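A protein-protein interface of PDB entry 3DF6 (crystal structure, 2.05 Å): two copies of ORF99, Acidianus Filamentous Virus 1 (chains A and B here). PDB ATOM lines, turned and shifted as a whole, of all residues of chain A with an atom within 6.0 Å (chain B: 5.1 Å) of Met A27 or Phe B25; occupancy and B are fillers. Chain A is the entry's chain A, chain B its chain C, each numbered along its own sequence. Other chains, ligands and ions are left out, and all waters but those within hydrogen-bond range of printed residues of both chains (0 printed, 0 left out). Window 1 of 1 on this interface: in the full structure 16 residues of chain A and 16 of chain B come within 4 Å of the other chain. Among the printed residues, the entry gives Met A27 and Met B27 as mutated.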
ATOM      1  N   LEU A   9      11.600 -20.437   8.190  1.00  0.00           N
ATOM      2  CA  LEU A   9      12.069 -21.250   7.061  1.00  0.00           C
ATOM      3  C   LEU A   9      11.349 -20.945   5.718  1.00  0.00           C
ATOM      4  O   LEU A   9      11.985 -20.893   4.671  1.00  0.00           O
ATOM      5  CB  LEU A   9      12.044 -22.740   7.415  1.00  0.00           C
ATOM      6  CG  LEU A   9      12.468 -23.654   6.265  1.00  0.00           C
ATOM      7  CD1 LEU A   9      13.289 -24.767   6.804  1.00  0.00           C
ATOM      8  CD2 LEU A   9      11.232 -24.166   5.487  1.00  0.00           C
ATOM      9  N   LEU A  10      10.035 -20.756   5.727  1.00  0.00           N
ATOM     10  CA  LEU A  10       9.341 -20.461   4.466  1.00  0.00           C
ATOM     11  C   LEU A  10       9.878 -19.165   3.870  1.00  0.00           C
ATOM     12  O   LEU A  10      10.114 -19.066   2.663  1.00  0.00           O
ATOM     13  CB  LEU A  10       7.825 -20.358   4.683  1.00  0.00           C
ATOM     14  CG  LEU A  10       7.147 -21.619   5.249  1.00  0.00           C
ATOM     15  CD1 LEU A  10       5.689 -21.294   5.517  1.00  0.00           C
ATOM     16  CD2 LEU A  10       7.267 -22.810   4.321  1.00  0.00           C
ATOM     17  N   VAL A  13      13.227 -19.838   2.396  1.00  0.00           N
ATOM     18  CA  VAL A  13      13.068 -20.566   1.107  1.00  0.00           C
ATOM     19  C   VAL A  13      12.846 -19.565  -0.042  1.00  0.00           C
ATOM     20  O   VAL A  13      13.512 -19.640  -1.089  1.00  0.00           O
ATOM     21  CB  VAL A  13      11.918 -21.619   1.143  1.00  0.00           C
ATOM     22  CG1 VAL A  13      11.529 -22.055  -0.292  1.00  0.00           C
ATOM     23  CG2 VAL A  13      12.320 -22.836   2.002  1.00  0.00           C
ATOM     24  N   VAL A  14      11.903 -18.638   0.150  1.00  0.00           N
ATOM     25  CA  VAL A  14      11.680 -17.562  -0.825  1.00  0.00           C
ATOM     26  C   VAL A  14      12.967 -16.751  -1.078  1.00  0.00           C
ATOM     27  O   VAL A  14      13.311 -16.499  -2.229  1.00  0.00           O
ATOM     28  CB  VAL A  14      10.475 -16.673  -0.432  1.00  0.00           C
ATOM     29  CG1 VAL A  14      10.344 -15.495  -1.353  1.00  0.00           C
ATOM     30  CG2 VAL A  14       9.175 -17.526  -0.455  1.00  0.00           C
ATOM     31  N   PHE A  25      10.623 -23.687  -7.238  1.00  0.00           N
ATOM     32  CA  PHE A  25      10.087 -24.570  -6.184  1.00  0.00           C
ATOM     33  C   PHE A  25       8.572 -24.473  -6.093  1.00  0.00           C
ATOM     34  O   PHE A  25       7.957 -23.515  -6.592  1.00  0.00           O
ATOM     35  CB  PHE A  25      10.699 -24.206  -4.796  1.00  0.00           C
ATOM     36  CG  PHE A  25      10.096 -22.968  -4.181  1.00  0.00           C
ATOM     37  CD1 PHE A  25       9.009 -23.059  -3.289  1.00  0.00           C
ATOM     38  CD2 PHE A  25      10.563 -21.706  -4.536  1.00  0.00           C
ATOM     39  CE1 PHE A  25       8.418 -21.888  -2.744  1.00  0.00           C
ATOM     40  CE2 PHE A  25       9.988 -20.547  -4.005  1.00  0.00           C
ATOM     41  CZ  PHE A  25       8.913 -20.640  -3.103  1.00  0.00           C
ATOM     42  N   GLU A  26       7.966 -25.443  -5.423  1.00  0.00           N
ATOM     43  CA  GLU A  26       6.573 -25.299  -5.006  1.00  0.00           C
ATOM     44  C   GLU A  26       6.492 -25.938  -3.658  1.00  0.00           C
ATOM     45  O   GLU A  26       7.221 -26.897  -3.390  1.00  0.00           O
ATOM     46  CB  GLU A  26       5.613 -26.095  -5.881  1.00  0.00           C
ATOM     47  CG  GLU A  26       5.623 -25.823  -7.300  1.00  0.00           C
ATOM     48  CD  GLU A  26       4.511 -26.590  -7.997  1.00  0.00           C
ATOM     49  OE1 GLU A  26       4.113 -27.666  -7.500  1.00  0.00           O
ATOM     50  OE2 GLU A  26       4.049 -26.128  -9.033  1.00  0.00           O
ATOM     51  N   MET A  27       5.590 -25.427  -2.829  1.00  0.00           N
ATOM     52  CA  MET A  27       5.231 -26.077  -1.565  1.00  0.00           C
ATOM     53  C   MET A  27       3.719 -25.997  -1.378  1.00  0.00           C
ATOM     54  O   MET A  27       3.109 -24.923  -1.573  1.00  0.00           O
ATOM     55  CB  MET A  27       5.909 -25.393  -0.393  1.00  0.00           C
ATOM     56  CG  MET A  27       7.415 -25.554  -0.352  1.00  0.00           C
ATOM     57  SD  MET A  27       8.168 -24.700   1.203  1.00  0.00           S
ATOM     58  CE  MET A  27       8.013 -22.825   0.711  1.00  0.00           C
ATOM     59  N   LYS A  28       3.134 -27.131  -1.004  1.00  0.00           N
ATOM     60  CA  LYS A  28       1.752 -27.203  -0.563  1.00  0.00           C
ATOM     61  C   LYS A  28       1.736 -27.100   0.976  1.00  0.00           C
ATOM     62  O   LYS A  28       2.500 -27.803   1.667  1.00  0.00           O
ATOM     63  CB  LYS A  28       1.119 -28.520  -1.027  1.00  0.00           C
ATOM     64  CG  LYS A  28      -0.337 -28.668  -0.608  1.00  0.00           C
ATOM     65  CD  LYS A  28      -0.901 -30.020  -1.077  1.00  0.00           C
ATOM     66  CE  LYS A  28      -2.340 -30.177  -0.586  1.00  0.00           C
ATOM     67  NZ  LYS A  28      -3.132 -29.007  -0.942  1.00  0.00           N
ATOM     68  N   LEU A  29       0.848 -26.258   1.497  1.00  0.00           N
ATOM     69  CA  LEU A  29       0.886 -25.882   2.899  1.00  0.00           C
ATOM     70  C   LEU A  29      -0.485 -25.624   3.466  1.00  0.00           C
ATOM     71  O   LEU A  29      -1.400 -25.257   2.726  1.00  0.00           O
ATOM     72  CB  LEU A  29       1.592 -24.517   3.042  1.00  0.00           C
ATOM     73  CG  LEU A  29       3.054 -24.398   2.578  1.00  0.00           C
ATOM     74  CD1 LEU A  29       3.520 -22.955   2.545  1.00  0.00           C
ATOM     75  CD2 LEU A  29       3.984 -25.240   3.431  1.00  0.00           C
ATOM     76  N   LEU A  88      -1.923 -21.628   1.492  1.00  0.00           N
ATOM     77  CA  LEU A  88      -2.173 -22.966   0.960  1.00  0.00           C
ATOM     78  C   LEU A  88      -1.115 -23.475  -0.024  1.00  0.00           C
ATOM     79  O   LEU A  88      -0.914 -24.685  -0.126  1.00  0.00           O
ATOM     80  CB  LEU A  88      -3.543 -23.019   0.280  1.00  0.00           C
ATOM     81  CG  LEU A  88      -4.738 -22.629   1.160  1.00  0.00           C
ATOM     82  CD1 LEU A  88      -6.007 -22.727   0.317  1.00  0.00           C
ATOM     83  CD2 LEU A  88      -4.836 -23.487   2.412  1.00  0.00           C
ATOM     84  N   SER A  89      -0.498 -22.566  -0.772  1.00  0.00           N
ATOM     85  CA  SER A  89       0.676 -22.914  -1.572  1.00  0.00           C
ATOM     86  C   SER A  89       1.576 -21.719  -1.821  1.00  0.00           C
ATOM     87  O   SER A  89       1.133 -20.574  -1.820  1.00  0.00           O
ATOM     88  CB  SER A  89       0.305 -23.598  -2.911  1.00  0.00           C
ATOM     89  OG  SER A  89      -0.387 -22.695  -3.749  1.00  0.00           O
ATOM     90  N   ILE A  90       2.861 -22.011  -2.019  1.00  0.00           N
ATOM     91  CA  ILE A  90       3.827 -21.015  -2.457  1.00  0.00           C
ATOM     92  C   ILE A  90       4.594 -21.638  -3.605  1.00  0.00           C
ATOM     93  O   ILE A  90       5.049 -22.794  -3.504  1.00  0.00           O
ATOM     94  CB  ILE A  90       4.792 -20.607  -1.331  1.00  0.00           C
ATOM     95  CG1 ILE A  90       4.033 -20.019  -0.138  1.00  0.00           C
ATOM     96  CG2 ILE A  90       5.818 -19.562  -1.830  1.00  0.00           C
ATOM     97  CD1 ILE A  90       4.927 -19.824   1.128  1.00  0.00           C
ATOM     98  N   LYS A  91       4.720 -20.890  -4.700  1.00  0.00           N
ATOM     99  CA  LYS A  91       5.405 -21.383  -5.896  1.00  0.00           C
ATOM    100  C   LYS A  91       6.314 -20.290  -6.434  1.00  0.00           C
ATOM    101  O   LYS A  91       5.870 -19.128  -6.601  1.00  0.00           O
ATOM    102  CB  LYS A  91       4.395 -21.762  -6.982  1.00  0.00           C
ATOM    103  CG  LYS A  91       5.006 -22.402  -8.229  1.00  0.00           C
ATOM    104  CD  LYS A  91       3.916 -22.965  -9.138  1.00  0.00           C
ATOM    105  CE  LYS A  91       4.471 -23.572 -10.456  1.00  0.00           C
ATOM    106  NZ  LYS A  91       5.495 -24.628 -10.271  1.00  0.00           N
ATOM    107  N   VAL B  13      13.796 -28.799   5.278  1.00  0.00           N
ATOM    108  CA  VAL B  13      12.651 -28.883   4.357  1.00  0.00           C
ATOM    109  C   VAL B  13      12.142 -30.321   4.336  1.00  0.00           C
ATOM    110  O   VAL B  13      10.934 -30.559   4.486  1.00  0.00           O
ATOM    111  CB  VAL B  13      12.997 -28.358   2.918  1.00  0.00           C
ATOM    112  CG1 VAL B  13      11.915 -28.753   1.863  1.00  0.00           C
ATOM    113  CG2 VAL B  13      13.195 -26.825   2.923  1.00  0.00           C
ATOM    114  N   VAL B  14      13.059 -31.274   4.174  1.00  0.00           N
ATOM    115  CA  VAL B  14      12.687 -32.691   4.109  1.00  0.00           C
ATOM    116  C   VAL B  14      12.080 -33.135   5.454  1.00  0.00           C
ATOM    117  O   VAL B  14      11.026 -33.787   5.483  1.00  0.00           O
ATOM    118  CB  VAL B  14      13.891 -33.591   3.623  1.00  0.00           C
ATOM    119  CG1 VAL B  14      13.595 -35.086   3.775  1.00  0.00           C
ATOM    120  CG2 VAL B  14      14.225 -33.272   2.186  1.00  0.00           C
ATOM    121  N   PHE B  17       8.592 -31.755   5.695  1.00  0.00           N
ATOM    122  CA  PHE B  17       7.785 -32.548   4.790  1.00  0.00           C
ATOM    123  C   PHE B  17       7.386 -33.869   5.450  1.00  0.00           C
ATOM    124  O   PHE B  17       6.197 -34.227   5.454  1.00  0.00           O
ATOM    125  CB  PHE B  17       8.516 -32.770   3.445  1.00  0.00           C
ATOM    126  CG  PHE B  17       7.935 -33.890   2.618  1.00  0.00           C
ATOM    127  CD1 PHE B  17       6.672 -33.758   2.035  1.00  0.00           C
ATOM    128  CD2 PHE B  17       8.638 -35.082   2.454  1.00  0.00           C
ATOM    129  CE1 PHE B  17       6.106 -34.796   1.285  1.00  0.00           C
ATOM    130  CE2 PHE B  17       8.092 -36.137   1.693  1.00  0.00           C
ATOM    131  CZ  PHE B  17       6.818 -35.999   1.120  1.00  0.00           C
ATOM    132  N   ILE B  22       5.108 -29.298   5.811  1.00  0.00           N
ATOM    133  CA  ILE B  22       5.114 -29.158   4.355  1.00  0.00           C
ATOM    134  C   ILE B  22       4.379 -30.399   3.852  1.00  0.00           C
ATOM    135  O   ILE B  22       4.823 -31.521   4.080  1.00  0.00           O
ATOM    136  CB  ILE B  22       6.520 -29.027   3.766  1.00  0.00           C
ATOM    137  CG1 ILE B  22       7.184 -27.705   4.224  1.00  0.00           C
ATOM    138  CG2 ILE B  22       6.476 -29.061   2.231  1.00  0.00           C
ATOM    139  CD1 ILE B  22       8.727 -27.694   4.008  1.00  0.00           C
ATOM    140  N   LYS B  23       3.214 -30.198   3.236  1.00  0.00           N
ATOM    141  CA  LYS B  23       2.401 -31.322   2.788  1.00  0.00           C
ATOM    142  C   LYS B  23       3.083 -32.031   1.606  1.00  0.00           C
ATOM    143  O   LYS B  23       3.196 -33.261   1.606  1.00  0.00           O
ATOM    144  CB  LYS B  23       1.017 -30.847   2.349  1.00  0.00           C
ATOM    145  CG  LYS B  23       0.275 -29.929   3.341  1.00  0.00           C
ATOM    146  CD  LYS B  23       0.154 -30.537   4.709  1.00  0.00           C
ATOM    147  CE  LYS B  23      -0.360 -29.496   5.728  1.00  0.00           C
ATOM    148  NZ  LYS B  23      -0.329 -30.049   7.096  1.00  0.00           N
ATOM    149  N   GLU B  24       3.473 -31.243   0.595  1.00  0.00           N
ATOM    150  CA  GLU B  24       4.203 -31.724  -0.596  1.00  0.00           C
ATOM    151  C   GLU B  24       5.089 -30.589  -1.095  1.00  0.00           C
ATOM    152  O   GLU B  24       4.837 -29.421  -0.781  1.00  0.00           O
ATOM    153  CB  GLU B  24       3.222 -32.108  -1.725  1.00  0.00           C
ATOM    154  CG  GLU B  24       2.308 -33.285  -1.357  1.00  0.00           C
ATOM    155  CD  GLU B  24       1.602 -33.841  -2.564  1.00  0.00           C
ATOM    156  OE1 GLU B  24       1.098 -33.024  -3.365  1.00  0.00           O
ATOM    157  OE2 GLU B  24       1.563 -35.093  -2.720  1.00  0.00           O
ATOM    158  N   PHE B  25       6.101 -30.902  -1.891  1.00  0.00           N
ATOM    159  CA  PHE B  25       6.984 -29.833  -2.388  1.00  0.00           C
ATOM    160  C   PHE B  25       7.809 -30.371  -3.535  1.00  0.00           C
ATOM    161  O   PHE B  25       7.877 -31.588  -3.751  1.00  0.00           O
ATOM    162  CB  PHE B  25       7.919 -29.298  -1.270  1.00  0.00           C
ATOM    163  CG  PHE B  25       9.079 -30.229  -0.951  1.00  0.00           C
ATOM    164  CD1 PHE B  25      10.316 -30.060  -1.577  1.00  0.00           C
ATOM    165  CD2 PHE B  25       8.911 -31.302  -0.081  1.00  0.00           C
ATOM    166  CE1 PHE B  25      11.382 -30.950  -1.307  1.00  0.00           C
ATOM    167  CE2 PHE B  25       9.977 -32.202   0.186  1.00  0.00           C
ATOM    168  CZ  PHE B  25      11.198 -32.011  -0.424  1.00  0.00           C
ATOM    169  N   GLU B  26       8.415 -29.454  -4.278  1.00  0.00           N
ATOM    170  CA  GLU B  26       9.465 -29.784  -5.228  1.00  0.00           C
ATOM    171  C   GLU B  26      10.405 -28.595  -5.293  1.00  0.00           C
ATOM    172  O   GLU B  26       9.985 -27.446  -5.124  1.00  0.00           O
ATOM    173  CB  GLU B  26       8.893 -30.090  -6.620  1.00  0.00           C
ATOM    174  CG  GLU B  26       8.188 -28.939  -7.270  1.00  0.00           C
ATOM    175  CD  GLU B  26       7.532 -29.335  -8.601  1.00  0.00           C
ATOM    176  OE1 GLU B  26       7.899 -30.391  -9.188  1.00  0.00           O
ATOM    177  OE2 GLU B  26       6.679 -28.553  -9.068  1.00  0.00           O
ATOM    178  N   MET B  27      11.675 -28.863  -5.528  1.00  0.00           N
ATOM    179  CA  MET B  27      12.668 -27.800  -5.640  1.00  0.00           C
ATOM    180  C   MET B  27      13.659 -28.222  -6.711  1.00  0.00           C
ATOM    181  O   MET B  27      14.087 -29.380  -6.738  1.00  0.00           O
ATOM    182  CB  MET B  27      13.441 -27.614  -4.342  1.00  0.00           C
ATOM    183  CG  MET B  27      12.682 -27.062  -3.175  1.00  0.00           C
ATOM    184  SD  MET B  27      13.978 -26.885  -1.728  1.00  0.00           S
ATOM    185  CE  MET B  27      14.423 -28.739  -1.380  1.00  0.00           C
ATOM    186  N   LEU B  73       9.846 -39.398  -1.148  1.00  0.00           N
ATOM    187  CA  LEU B  73      10.868 -38.406  -1.466  1.00  0.00           C
ATOM    188  C   LEU B  73      11.656 -38.827  -2.702  1.00  0.00           C
ATOM    189  O   LEU B  73      12.226 -39.915  -2.750  1.00  0.00           O
ATOM    190  CB  LEU B  73      11.826 -38.257  -0.272  1.00  0.00           C
ATOM    191  CG  LEU B  73      12.832 -37.108  -0.387  1.00  0.00           C
ATOM    192  CD1 LEU B  73      12.089 -35.745  -0.124  1.00  0.00           C
ATOM    193  CD2 LEU B  73      14.017 -37.314   0.535  1.00  0.00           C
ATOM    194  N   ILE B  90      14.686 -32.197  -5.721  1.00  0.00           N
ATOM    195  CA  ILE B  90      14.105 -32.915  -4.614  1.00  0.00           C
ATOM    196  C   ILE B  90      12.575 -32.692  -4.721  1.00  0.00           C
ATOM    197  O   ILE B  90      12.125 -31.562  -4.959  1.00  0.00           O
ATOM    198  CB  ILE B  90      14.617 -32.405  -3.222  1.00  0.00           C
ATOM    199  CG1 ILE B  90      16.149 -32.425  -3.147  1.00  0.00           C
ATOM    200  CG2 ILE B  90      14.066 -33.326  -2.103  1.00  0.00           C
ATOM    201  CD1 ILE B  90      16.789 -31.818  -1.820  1.00  0.00           C
ATOM    202  N   LYS B  91      11.798 -33.766  -4.570  1.00  0.00           N
ATOM    203  CA  LYS B  91      10.344 -33.698  -4.635  1.00  0.00           C
ATOM    204  C   LYS B  91       9.734 -34.583  -3.563  1.00  0.00           C
ATOM    205  O   LYS B  91      10.161 -35.737  -3.378  1.00  0.00           O
ATOM    206  CB  LYS B  91       9.841 -34.122  -6.011  1.00  0.00           C
ATOM    207  CG  LYS B  91       8.308 -34.070  -6.202  1.00  0.00           C
ATOM    208  CD  LYS B  91       7.962 -34.460  -7.653  1.00  0.00           C
ATOM    209  CE  LYS B  91       6.457 -34.528  -7.926  1.00  0.00           C
ATOM    210  NZ  LYS B  91       5.753 -33.286  -7.469  1.00  0.00           N
ATOM    211  N   GLY B  92       8.742 -34.032  -2.858  1.00  0.00           N
ATOM    212  CA  GLY B  92       8.071 -34.741  -1.770  1.00  0.00           C
ATOM    213  C   GLY B  92       6.602 -34.869  -2.117  1.00  0.00           C
ATOM    214  O   GLY B  92       5.949 -33.876  -2.430  1.00  0.00           O
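O of Glu B26 is in hydrogen-bond range of N of Glu A26, 2.9 Å away. O of Lys A28 lies within hydrogen-bond range of N of Lys B23, 3.0 Å away. O of Glu B24 sits at hydrogen-bond distance from N of Lys A28 (2.9 Å).
NZ of Lys A91 is in salt-bridge range of OE2 of Glu A26, at 2.4 Å. The backbone carbonyl oxygen of Ile A90 sits at hydrogen-bond distance from the backbone NH of Met A27. O of Phe B25 sits at hydrogen-bond distance from N of Gly B92 (2.7 Å). OE1 of Glu B26 is in salt-bridge range of NZ of Lys B91, 3.99 Å away. The backbone NH (N) of Met B27 lies within hydrogen-bond range of the backbone carbonyl oxygen (O) of Ile B90 (2.8 Å).
Phe A25 touches Glu B26. Phe A25 touches Met B27. Glu A26 touches Phe B25. Met A27 touches Glu B24. Phe B25 touches Met A27. Lys A28 touches Ile B22 (O to C, 3.9 Å).
Printed residues of chain B within 4 Å of Met A27: Glu B24 and Phe B25. Printed residues of chain A within 4 Å of Ile B22: Lys A28 (3.9 Å). Printed residues of chain A within 4 Å of Lys B23: Lys A28. Of chain A, only Glu A26 and Met A27 come within 4 Å of Phe B25.
Of the 13 printed residues of chain B, 6 touch a printed residue of chain A. Hydrophobic or aromatic side chains of chain B within 4 Å of the printed part of chain A: Phe B25 and Met B27. Hydrophobic or aromatic side chains of chain A that line the printed part of chain B: Phe A25 and Met A27. Among the printed residues, 9 pairs touch across the chains. Among the printed residues, no Asp or Glu carboxylate lies within 4 Å of a Lys or Arg side-chain nitrogen of the other chain.
Phe A25 touches Glu B26, and with the chains exchanged Glu A26 touches Phe B25. Phe A25 touches Met B27, and with the chains exchanged Met A27 touches Phe B25. Glu A26 touches its own counterpart, Glu B26. 7 positions are printed for both chains. Of the 9 pairs that touch across the chains among the printed residues, 5 have their exchanged pair printed and touching as well.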
